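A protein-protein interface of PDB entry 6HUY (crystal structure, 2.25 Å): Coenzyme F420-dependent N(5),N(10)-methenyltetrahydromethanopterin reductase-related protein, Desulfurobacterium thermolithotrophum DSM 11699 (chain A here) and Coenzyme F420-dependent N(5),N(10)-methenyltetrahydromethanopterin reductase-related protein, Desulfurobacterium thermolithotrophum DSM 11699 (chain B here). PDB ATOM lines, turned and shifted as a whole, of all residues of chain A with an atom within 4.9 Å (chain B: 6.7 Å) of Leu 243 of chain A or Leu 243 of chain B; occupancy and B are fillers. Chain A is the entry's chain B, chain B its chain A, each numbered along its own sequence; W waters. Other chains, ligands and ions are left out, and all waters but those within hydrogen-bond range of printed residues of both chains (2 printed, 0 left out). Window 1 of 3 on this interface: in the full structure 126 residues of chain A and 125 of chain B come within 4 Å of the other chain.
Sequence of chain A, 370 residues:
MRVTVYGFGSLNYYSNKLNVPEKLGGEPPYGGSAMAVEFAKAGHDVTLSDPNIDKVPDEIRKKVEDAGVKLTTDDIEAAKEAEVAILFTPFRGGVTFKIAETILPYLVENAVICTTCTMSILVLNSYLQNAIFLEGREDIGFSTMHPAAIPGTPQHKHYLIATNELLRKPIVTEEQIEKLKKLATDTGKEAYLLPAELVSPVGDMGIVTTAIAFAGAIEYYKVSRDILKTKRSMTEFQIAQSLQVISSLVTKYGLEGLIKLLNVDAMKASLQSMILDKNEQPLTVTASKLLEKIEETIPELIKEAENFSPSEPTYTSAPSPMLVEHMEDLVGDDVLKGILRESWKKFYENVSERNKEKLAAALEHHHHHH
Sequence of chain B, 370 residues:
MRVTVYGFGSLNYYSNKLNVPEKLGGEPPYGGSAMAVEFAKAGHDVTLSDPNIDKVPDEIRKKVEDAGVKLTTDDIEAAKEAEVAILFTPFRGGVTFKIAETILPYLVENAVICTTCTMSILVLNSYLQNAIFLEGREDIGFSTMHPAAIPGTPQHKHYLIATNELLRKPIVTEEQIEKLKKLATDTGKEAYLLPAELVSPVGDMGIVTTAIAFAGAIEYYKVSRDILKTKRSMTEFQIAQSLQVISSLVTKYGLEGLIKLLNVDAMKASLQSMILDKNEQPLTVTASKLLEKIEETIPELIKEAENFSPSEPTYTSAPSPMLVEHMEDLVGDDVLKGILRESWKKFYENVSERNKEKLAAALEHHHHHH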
ATOM      1  N   THR A 209      15.274 -21.265 -18.047  1.00  0.00           N
ATOM      2  CA  THR A 209      16.446 -22.022 -18.482  1.00  0.00           C
ATOM      3  C   THR A 209      17.609 -21.862 -17.508  1.00  0.00           C
ATOM      4  O   THR A 209      18.352 -22.823 -17.259  1.00  0.00           O
ATOM      5  CB  THR A 209      16.851 -21.584 -19.893  1.00  0.00           C
ATOM      6  OG1 THR A 209      15.769 -21.840 -20.804  1.00  0.00           O
ATOM      7  CG2 THR A 209      18.063 -22.329 -20.393  1.00  0.00           C
ATOM      8  N   ALA A 213      18.964 -25.179 -15.526  1.00  0.00           N
ATOM      9  CA  ALA A 213      20.352 -25.547 -15.777  1.00  0.00           C
ATOM     10  C   ALA A 213      21.181 -25.484 -14.499  1.00  0.00           C
ATOM     11  O   ALA A 213      22.068 -26.319 -14.289  1.00  0.00           O
ATOM     12  CB  ALA A 213      20.956 -24.629 -16.848  1.00  0.00           C
ATOM     13  N   ILE A 239      30.261 -29.617 -16.278  1.00  0.00           N
ATOM     14  CA  ILE A 239      29.180 -28.649 -16.166  1.00  0.00           C
ATOM     15  C   ILE A 239      29.423 -27.496 -17.122  1.00  0.00           C
ATOM     16  O   ILE A 239      28.537 -27.099 -17.884  1.00  0.00           O
ATOM     17  CB  ILE A 239      29.047 -28.156 -14.714  1.00  0.00           C
ATOM     18  CG1 ILE A 239      28.429 -29.242 -13.833  1.00  0.00           C
ATOM     19  CG2 ILE A 239      28.208 -26.890 -14.640  1.00  0.00           C
ATOM     20  CD1 ILE A 239      28.634 -28.990 -12.335  1.00  0.00           C
ATOM     21  N   ALA A 240      30.631 -26.935 -17.090  1.00  0.00           N
ATOM     22  CA  ALA A 240      30.905 -25.779 -17.932  1.00  0.00           C
ATOM     23  C   ALA A 240      30.797 -26.143 -19.403  1.00  0.00           C
ATOM     24  O   ALA A 240      30.235 -25.377 -20.196  1.00  0.00           O
ATOM     25  CB  ALA A 240      32.281 -25.209 -17.614  1.00  0.00           C
ATOM     26  N   GLN A 241      31.294 -27.321 -19.787  1.00  0.00           N
ATOM     27  CA  GLN A 241      31.275 -27.698 -21.194  1.00  0.00           C
ATOM     28  C   GLN A 241      29.841 -27.865 -21.686  1.00  0.00           C
ATOM     29  O   GLN A 241      29.472 -27.367 -22.759  1.00  0.00           O
ATOM     30  CB  GLN A 241      32.082 -28.980 -21.413  1.00  0.00           C
ATOM     31  CG  GLN A 241      31.991 -29.520 -22.860  1.00  0.00           C
ATOM     32  CD  GLN A 241      32.826 -30.755 -23.097  1.00  0.00           C
ATOM     33  OE1 GLN A 241      33.805 -30.736 -23.846  1.00  0.00           O
ATOM     34  NE2 GLN A 241      32.436 -31.847 -22.463  1.00  0.00           N
ATOM     35  N   SER A 242      29.007 -28.546 -20.895  1.00  0.00           N
ATOM     36  CA  SER A 242      27.618 -28.769 -21.289  1.00  0.00           C
ATOM     37  C   SER A 242      26.911 -27.456 -21.581  1.00  0.00           C
ATOM     38  O   SER A 242      26.236 -27.312 -22.606  1.00  0.00           O
ATOM     39  CB  SER A 242      26.858 -29.529 -20.193  1.00  0.00           C
ATOM     40  OG  SER A 242      27.431 -30.800 -19.971  1.00  0.00           O
ATOM     41  N   LEU A 243      27.038 -26.490 -20.672  1.00  0.00           N
ATOM     42  CA  LEU A 243      26.269 -25.258 -20.789  1.00  0.00           C
ATOM     43  C   LEU A 243      26.847 -24.340 -21.855  1.00  0.00           C
ATOM     44  O   LEU A 243      26.089 -23.658 -22.555  1.00  0.00           O
ATOM     45  CB  LEU A 243      26.206 -24.549 -19.434  1.00  0.00           C
ATOM     46  CG  LEU A 243      25.670 -25.394 -18.270  1.00  0.00           C
ATOM     47  CD1 LEU A 243      25.675 -24.590 -16.975  1.00  0.00           C
ATOM     48  CD2 LEU A 243      24.259 -25.912 -18.549  1.00  0.00           C
ATOM     49  N   GLN A 244      28.176 -24.326 -22.005  1.00  0.00           N
ATOM     50  CA  GLN A 244      28.796 -23.566 -23.084  1.00  0.00           C
ATOM     51  C   GLN A 244      28.379 -24.121 -24.447  1.00  0.00           C
ATOM     52  O   GLN A 244      28.033 -23.360 -25.362  1.00  0.00           O
ATOM     53  CB  GLN A 244      30.313 -23.592 -22.928  1.00  0.00           C
ATOM     54  CG  GLN A 244      31.079 -22.854 -24.011  1.00  0.00           C
ATOM     55  CD  GLN A 244      30.757 -21.365 -24.021  1.00  0.00           C
ATOM     56  OE1 GLN A 244      31.361 -20.572 -23.284  1.00  0.00           O
ATOM     57  NE2 GLN A 244      29.788 -20.983 -24.845  1.00  0.00           N
ATOM     58  N   VAL A 245      28.369 -25.448 -24.587  1.00  0.00           N
ATOM     59  CA  VAL A 245      27.968 -26.061 -25.846  1.00  0.00           C
ATOM     60  C   VAL A 245      26.549 -25.638 -26.216  1.00  0.00           C
ATOM     61  O   VAL A 245      26.291 -25.193 -27.340  1.00  0.00           O
ATOM     62  CB  VAL A 245      28.113 -27.589 -25.752  1.00  0.00           C
ATOM     63  CG1 VAL A 245      27.336 -28.298 -26.841  1.00  0.00           C
ATOM     64  CG2 VAL A 245      29.571 -27.968 -25.831  1.00  0.00           C
ATOM     65  N   ILE A 246      25.611 -25.760 -25.280  1.00  0.00           N
ATOM     66  CA  ILE A 246      24.229 -25.421 -25.602  1.00  0.00           C
ATOM     67  C   ILE A 246      24.111 -23.946 -25.970  1.00  0.00           C
ATOM     68  O   ILE A 246      23.430 -23.590 -26.939  1.00  0.00           O
ATOM     69  CB  ILE A 246      23.296 -25.811 -24.443  1.00  0.00           C
ATOM     70  CG1 ILE A 246      23.267 -27.336 -24.309  1.00  0.00           C
ATOM     71  CG2 ILE A 246      21.873 -25.297 -24.687  1.00  0.00           C
ATOM     72  CD1 ILE A 246      22.776 -27.843 -22.977  1.00  0.00           C
ATOM     73  N   SER A 247      24.780 -23.070 -25.216  1.00  0.00           N
ATOM     74  CA  SER A 247      24.759 -21.645 -25.531  1.00  0.00           C
ATOM     75  C   SER A 247      25.305 -21.380 -26.934  1.00  0.00           C
ATOM     76  O   SER A 247      24.698 -20.649 -27.723  1.00  0.00           O
ATOM     77  CB  SER A 247      25.571 -20.880 -24.488  1.00  0.00           C
ATOM     78  OG  SER A 247      25.749 -19.531 -24.868  1.00  0.00           O
ATOM     79  N   THR B 209      23.991 -32.783 -17.240  1.00  0.00           N
ATOM     80  CA  THR B 209      23.840 -31.341 -17.399  1.00  0.00           C
ATOM     81  C   THR B 209      23.423 -30.978 -18.823  1.00  0.00           C
ATOM     82  O   THR B 209      22.640 -30.048 -19.027  1.00  0.00           O
ATOM     83  CB  THR B 209      25.135 -30.633 -17.006  1.00  0.00           C
ATOM     84  OG1 THR B 209      25.429 -30.917 -15.629  1.00  0.00           O
ATOM     85  CG2 THR B 209      24.958 -29.121 -17.144  1.00  0.00           C
ATOM     86  N   THR B 210      23.928 -31.705 -19.819  1.00  0.00           N
ATOM     87  CA  THR B 210      23.571 -31.421 -21.206  1.00  0.00           C
ATOM     88  C   THR B 210      22.087 -31.650 -21.446  1.00  0.00           C
ATOM     89  O   THR B 210      21.403 -30.814 -22.045  1.00  0.00           O
ATOM     90  CB  THR B 210      24.411 -32.301 -22.132  1.00  0.00           C
ATOM     91  OG1 THR B 210      25.792 -32.094 -21.828  1.00  0.00           O
ATOM     92  CG2 THR B 210      24.151 -31.999 -23.601  1.00  0.00           C
ATOM     93  N   ALA B 213      19.787 -29.142 -19.193  1.00  0.00           N
ATOM     94  CA  ALA B 213      19.840 -27.789 -19.726  1.00  0.00           C
ATOM     95  C   ALA B 213      19.183 -27.717 -21.097  1.00  0.00           C
ATOM     96  O   ALA B 213      18.490 -26.743 -21.417  1.00  0.00           O
ATOM     97  CB  ALA B 213      21.286 -27.319 -19.796  1.00  0.00           C
ATOM     98  N   PHE B 214      19.386 -28.744 -21.920  1.00  0.00           N
ATOM     99  CA  PHE B 214      18.689 -28.823 -23.193  1.00  0.00           C
ATOM    100  C   PHE B 214      17.187 -28.872 -22.977  1.00  0.00           C
ATOM    101  O   PHE B 214      16.430 -28.137 -23.618  1.00  0.00           O
ATOM    102  CB  PHE B 214      19.150 -30.058 -23.961  1.00  0.00           C
ATOM    103  CG  PHE B 214      18.352 -30.334 -25.207  1.00  0.00           C
ATOM    104  CD1 PHE B 214      18.713 -29.763 -26.413  1.00  0.00           C
ATOM    105  CD2 PHE B 214      17.244 -31.161 -25.170  1.00  0.00           C
ATOM    106  CE1 PHE B 214      17.981 -30.015 -27.561  1.00  0.00           C
ATOM    107  CE2 PHE B 214      16.514 -31.422 -26.310  1.00  0.00           C
ATOM    108  CZ  PHE B 214      16.880 -30.843 -27.510  1.00  0.00           C
ATOM    109  N   ALA B 217      15.893 -25.591 -21.929  1.00  0.00           N
ATOM    110  CA  ALA B 217      15.798 -24.658 -23.046  1.00  0.00           C
ATOM    111  C   ALA B 217      14.531 -24.915 -23.853  1.00  0.00           C
ATOM    112  O   ALA B 217      13.845 -23.969 -24.255  1.00  0.00           O
ATOM    113  CB  ALA B 217      17.037 -24.773 -23.928  1.00  0.00           C
ATOM    114  N   GLN B 238      17.882 -15.036 -25.016  1.00  0.00           N
ATOM    115  CA  GLN B 238      17.968 -15.177 -23.563  1.00  0.00           C
ATOM    116  C   GLN B 238      18.550 -16.528 -23.169  1.00  0.00           C
ATOM    117  O   GLN B 238      19.306 -16.619 -22.198  1.00  0.00           O
ATOM    118  CB  GLN B 238      16.593 -14.958 -22.925  1.00  0.00           C
ATOM    119  CG  GLN B 238      16.092 -13.525 -23.106  1.00  0.00           C
ATOM    120  CD  GLN B 238      14.808 -13.206 -22.365  1.00  0.00           C
ATOM    121  OE1 GLN B 238      14.181 -14.072 -21.734  1.00  0.00           O
ATOM    122  NE2 GLN B 238      14.427 -11.933 -22.402  1.00  0.00           N
ATOM    123  N   ILE B 239      18.223 -17.589 -23.910  1.00  0.00           N
ATOM    124  CA  ILE B 239      18.808 -18.895 -23.620  1.00  0.00           C
ATOM    125  C   ILE B 239      20.322 -18.822 -23.738  1.00  0.00           C
ATOM    126  O   ILE B 239      21.060 -19.191 -22.815  1.00  0.00           O
ATOM    127  CB  ILE B 239      18.235 -19.973 -24.559  1.00  0.00           C
ATOM    128  CG1 ILE B 239      16.768 -20.262 -24.227  1.00  0.00           C
ATOM    129  CG2 ILE B 239      19.064 -21.290 -24.475  1.00  0.00           C
ATOM    130  CD1 ILE B 239      16.033 -21.021 -25.326  1.00  0.00           C
ATOM    131  N   ALA B 240      20.803 -18.352 -24.891  1.00  0.00           N
ATOM    132  CA  ALA B 240      22.232 -18.369 -25.188  1.00  0.00           C
ATOM    133  C   ALA B 240      23.005 -17.536 -24.187  1.00  0.00           C
ATOM    134  O   ALA B 240      24.068 -17.944 -23.701  1.00  0.00           O
ATOM    135  CB  ALA B 240      22.456 -17.844 -26.612  1.00  0.00           C
ATOM    136  N   GLN B 241      22.480 -16.350 -23.894  1.00  0.00           N
ATOM    137  CA  GLN B 241      23.096 -15.432 -22.951  1.00  0.00           C
ATOM    138  C   GLN B 241      23.152 -16.025 -21.548  1.00  0.00           C
ATOM    139  O   GLN B 241      24.178 -15.935 -20.863  1.00  0.00           O
ATOM    140  CB  GLN B 241      22.277 -14.144 -22.969  1.00  0.00           C
ATOM    141  CG  GLN B 241      22.636 -13.074 -21.995  1.00  0.00           C
ATOM    142  CD  GLN B 241      21.855 -11.790 -22.290  1.00  0.00           C
ATOM    143  OE1 GLN B 241      22.307 -10.917 -23.036  1.00  0.00           O
ATOM    144  NE2 GLN B 241      20.654 -11.703 -21.732  1.00  0.00           N
ATOM    145  N   SER B 242      22.044 -16.626 -21.098  1.00  0.00           N
ATOM    146  CA  SER B 242      22.000 -17.185 -19.754  1.00  0.00           C
ATOM    147  C   SER B 242      23.002 -18.325 -19.598  1.00  0.00           C
ATOM    148  O   SER B 242      23.758 -18.377 -18.616  1.00  0.00           O
ATOM    149  CB  SER B 242      20.583 -17.671 -19.434  1.00  0.00           C
ATOM    150  OG  SER B 242      19.678 -16.577 -19.431  1.00  0.00           O
ATOM    151  N   LEU B 243      23.004 -19.263 -20.549  1.00  0.00           N
ATOM    152  CA  LEU B 243      23.881 -20.419 -20.434  1.00  0.00           C
ATOM    153  C   LEU B 243      25.336 -20.036 -20.660  1.00  0.00           C
ATOM    154  O   LEU B 243      26.228 -20.638 -20.052  1.00  0.00           O
ATOM    155  CB  LEU B 243      23.411 -21.516 -21.395  1.00  0.00           C
ATOM    156  CG  LEU B 243      22.013 -22.078 -21.064  1.00  0.00           C
ATOM    157  CD1 LEU B 243      21.594 -23.220 -22.005  1.00  0.00           C
ATOM    158  CD2 LEU B 243      21.942 -22.578 -19.638  1.00  0.00           C
ATOM    159  N   GLN B 244      25.581 -19.000 -21.470  1.00  0.00           N
ATOM    160  CA  GLN B 244      26.926 -18.443 -21.608  1.00  0.00           C
ATOM    161  C   GLN B 244      27.456 -17.914 -20.278  1.00  0.00           C
ATOM    162  O   GLN B 244      28.613 -18.162 -19.917  1.00  0.00           O
ATOM    163  CB  GLN B 244      26.917 -17.314 -22.637  1.00  0.00           C
ATOM    164  CG  GLN B 244      28.257 -16.616 -22.794  1.00  0.00           C
ATOM    165  CD  GLN B 244      29.317 -17.538 -23.362  1.00  0.00           C
ATOM    166  OE1 GLN B 244      29.400 -17.707 -24.577  1.00  0.00           O
ATOM    167  NE2 GLN B 244      30.098 -18.173 -22.490  1.00  0.00           N
ATOM    168  N   VAL B 245      26.635 -17.169 -19.538  1.00  0.00           N
ATOM    169  CA  VAL B 245      27.095 -16.592 -18.277  1.00  0.00           C
ATOM    170  C   VAL B 245      27.371 -17.688 -17.251  1.00  0.00           C
ATOM    171  O   VAL B 245      28.422 -17.695 -16.601  1.00  0.00           O
ATOM    172  CB  VAL B 245      26.071 -15.557 -17.765  1.00  0.00           C
ATOM    173  CG1 VAL B 245      26.378 -15.096 -16.328  1.00  0.00           C
ATOM    174  CG2 VAL B 245      26.055 -14.368 -18.704  1.00  0.00           C
ATOM    175  N   ILE B 246      26.442 -18.635 -17.092  1.00  0.00           N
ATOM    176  CA  ILE B 246      26.637 -19.700 -16.104  1.00  0.00           C
ATOM    177  C   ILE B 246      27.891 -20.497 -16.419  1.00  0.00           C
ATOM    178  O   ILE B 246      28.634 -20.911 -15.519  1.00  0.00           O
ATOM    179  CB  ILE B 246      25.419 -20.635 -16.058  1.00  0.00           C
ATOM    180  CG1 ILE B 246      24.171 -19.900 -15.590  1.00  0.00           C
ATOM    181  CG2 ILE B 246      25.719 -21.867 -15.139  1.00  0.00           C
ATOM    182  CD1 ILE B 246      22.933 -20.747 -15.809  1.00  0.00           C
ATOM    183  N   SER B 247      28.119 -20.761 -17.706  1.00  0.00           N
ATOM    184  CA  SER B 247      29.292 -21.514 -18.117  1.00  0.00           C
ATOM    185  C   SER B 247      30.568 -20.781 -17.735  1.00  0.00           C
ATOM    186  O   SER B 247      31.505 -21.373 -17.187  1.00  0.00           O
ATOM    187  CB  SER B 247      29.239 -21.758 -19.625  1.00  0.00           C
ATOM    188  OG  SER B 247      30.316 -22.587 -20.004  1.00  0.00           O
ATOM    189  N   SER B 248      30.633 -19.489 -18.045  1.00  0.00           N
ATOM    190  CA  SER B 248      31.817 -18.710 -17.709  1.00  0.00           C
ATOM    191  C   SER B 248      32.031 -18.664 -16.205  1.00  0.00           C
ATOM    192  O   SER B 248      33.167 -18.755 -15.729  1.00  0.00           O
ATOM    193  CB  SER B 248      31.676 -17.299 -18.252  1.00  0.00           C
ATOM    194  OG  SER B 248      31.558 -17.289 -19.658  1.00  0.00           O
ATOM    195  N   VAL B 250      31.258 -20.908 -13.971  1.00  0.00           N
ATOM    196  CA  VAL B 250      31.815 -22.174 -13.498  1.00  0.00           C
ATOM    197  C   VAL B 250      33.275 -22.313 -13.916  1.00  0.00           C
ATOM    198  O   VAL B 250      34.130 -22.712 -13.114  1.00  0.00           O
ATOM    199  CB  VAL B 250      30.979 -23.357 -14.001  1.00  0.00           C
ATOM    200  CG1 VAL B 250      31.674 -24.665 -13.634  1.00  0.00           C
ATOM    201  CG2 VAL B 250      29.583 -23.302 -13.417  1.00  0.00           C
ATOM    202  N   LEU B 258      29.896 -19.579  -8.692  1.00  0.00           N
ATOM    203  CA  LEU B 258      28.574 -19.544  -9.298  1.00  0.00           C
ATOM    204  C   LEU B 258      27.515 -19.264  -8.244  1.00  0.00           C
ATOM    205  O   LEU B 258      26.694 -18.352  -8.391  1.00  0.00           O
ATOM    206  CB  LEU B 258      28.285 -20.868  -9.996  1.00  0.00           C
ATOM    207  CG  LEU B 258      26.879 -20.984 -10.574  1.00  0.00           C
ATOM    208  CD1 LEU B 258      26.732 -20.073 -11.761  1.00  0.00           C
ATOM    209  CD2 LEU B 258      26.614 -22.400 -10.957  1.00  0.00           C
ATOM    210  N   THR B 316      31.760 -12.547 -18.466  1.00  0.00           N
ATOM    211  CA  THR B 316      31.114 -13.854 -18.452  1.00  0.00           C
ATOM    212  C   THR B 316      30.149 -14.019 -19.617  1.00  0.00           C
ATOM    213  O   THR B 316      29.832 -15.150 -20.005  1.00  0.00           O
ATOM    214  CB  THR B 316      30.366 -14.059 -17.135  1.00  0.00           C
ATOM    215  OG1 THR B 316      29.431 -12.993 -16.918  1.00  0.00           O
ATOM    216  CG2 THR B 316      31.337 -14.102 -15.982  1.00  0.00           C
HETATM  217  O   HOH W   1      32.387 -20.042 -21.137  1.00  0.00           O
HETATM  218  O   HOH W   2      27.313 -17.929 -26.648  1.00  0.00           O
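The backbone carbonyl oxygen (O) of Gln 244 of chain B is in hydrogen-bond range of the side-chain hydroxyl (OG) of Ser 248 of chain B.
The side-chain hydroxyl (OG) of Ser 242 of chain A lies within hydrogen-bond range of the side-chain hydroxyl (OG1) of Thr 210 of chain B (2.8 Å).
The side-chain hydroxyl (OG) of Ser 247 of chain A sits at hydrogen-bond distance from the backbone carbonyl oxygen (O) of Ala 240 of chain B (2.6 Å).
The side-chain amide nitrogen (NE2) of Gln 244 of chain B is in hydrogen-bond range of the side-chain amide oxygen (OE1) of Gln 244 of chain A.
OG of Ser 247 of chain A lies close to N of Gln 244 of chain B, 3.4 Å away.
The backbone carbonyl oxygen of Ala 240 of chain A is in hydrogen-bond range of the side-chain hydroxyl of Ser 247 of chain B (2.8 Å).
The side-chain hydroxyl (OG) of Ser 247 of chain B lies close to the backbone NH (N) of Gln 244 of chain A (3.4 Å).
Ala 217 of chain B touches Thr 209 of chain A (CA to OG1, 3.6 Å).
Thr 209 of chain A touches Ile 239 of chain B (OG1 to CG1, 3.9 Å).
OG1 of Thr 209 of chain B touches CG1 of Ile 239 of chain A (3.9 Å).
Ser 242 of chain A touches Thr 209 of chain B.
CG2 of Thr 209 of chain B touches CD2 of Leu 243 of chain A, 3.6 Å away.
Leu 243 of chain B touches Leu 243 of chain A (CB to O, 3.6 Å).
CD1 of Ile 246 of chain A touches CB of Ala 213 of chain B, at 3.6 Å.
Ile 246 of chain A touches Phe 214 of chain B (CD1 to N, 3.7 Å).
Leu 243 of chain B touches Ile 246 of chain A.
CB of Ser 247 of chain A touches CB of Leu 243 of chain B, 3.8 Å away.
Printed residues of chain A that touch a printed residue of chain B: Thr 209, Ala 213, Ile 239, Ala 240, Ser 242, Leu 243, Gln 244, Ile 246 and Ser 247.
Of the 19 printed residues of chain B, 11 touch a printed residue of chain A.
Hydrophobic or aromatic side chains of chain B within 4 Å of the printed part of chain A: Ala 213, Ile 239, Ala 240, Leu 243 and Ile 246.
Water W1 lies within hydrogen-bond range of the side-chain amide oxygen of Gln 244 of chain A (2.4 Å), the side-chain hydroxyl of Ser 248 of chain B (3.2 Å), the side-chain amide nitrogen of Gln 244 of chain B (3.3 Å) and the side-chain hydroxyl of Ser 247 of chain B (3.5 Å).
Water W2 bridges OG of Ser 247 of chain A (2.9 Å) and OE1 of Gln 244 of chain B (2.9 Å).
Of the printed residues of chain B, Ala 213 of chain A touches Leu 243.
Of chain B, only Thr 209, Ala 213, Leu 243 and Ile 246 come within 4 Å of Leu 243 of chain A.
Of the printed residues of chain A, Ala 213 of chain B touches Leu 243 (3.5 Å) and Ile 246 (3.6 Å).
Leu 243 of chain B touches just these residues of chain A: Thr 209 (3.96 Å), Ala 213 (3.6 Å), Leu 243 (3.6 Å), Ile 246 (3.4 Å) and Ser 247 (3.8 Å).
Val 250 of chain B touches none of the printed residues of chain A.
The nearest residue of chain B that does not touch Leu 243 of chain A is Ser 247 of chain B (4.1 Å).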
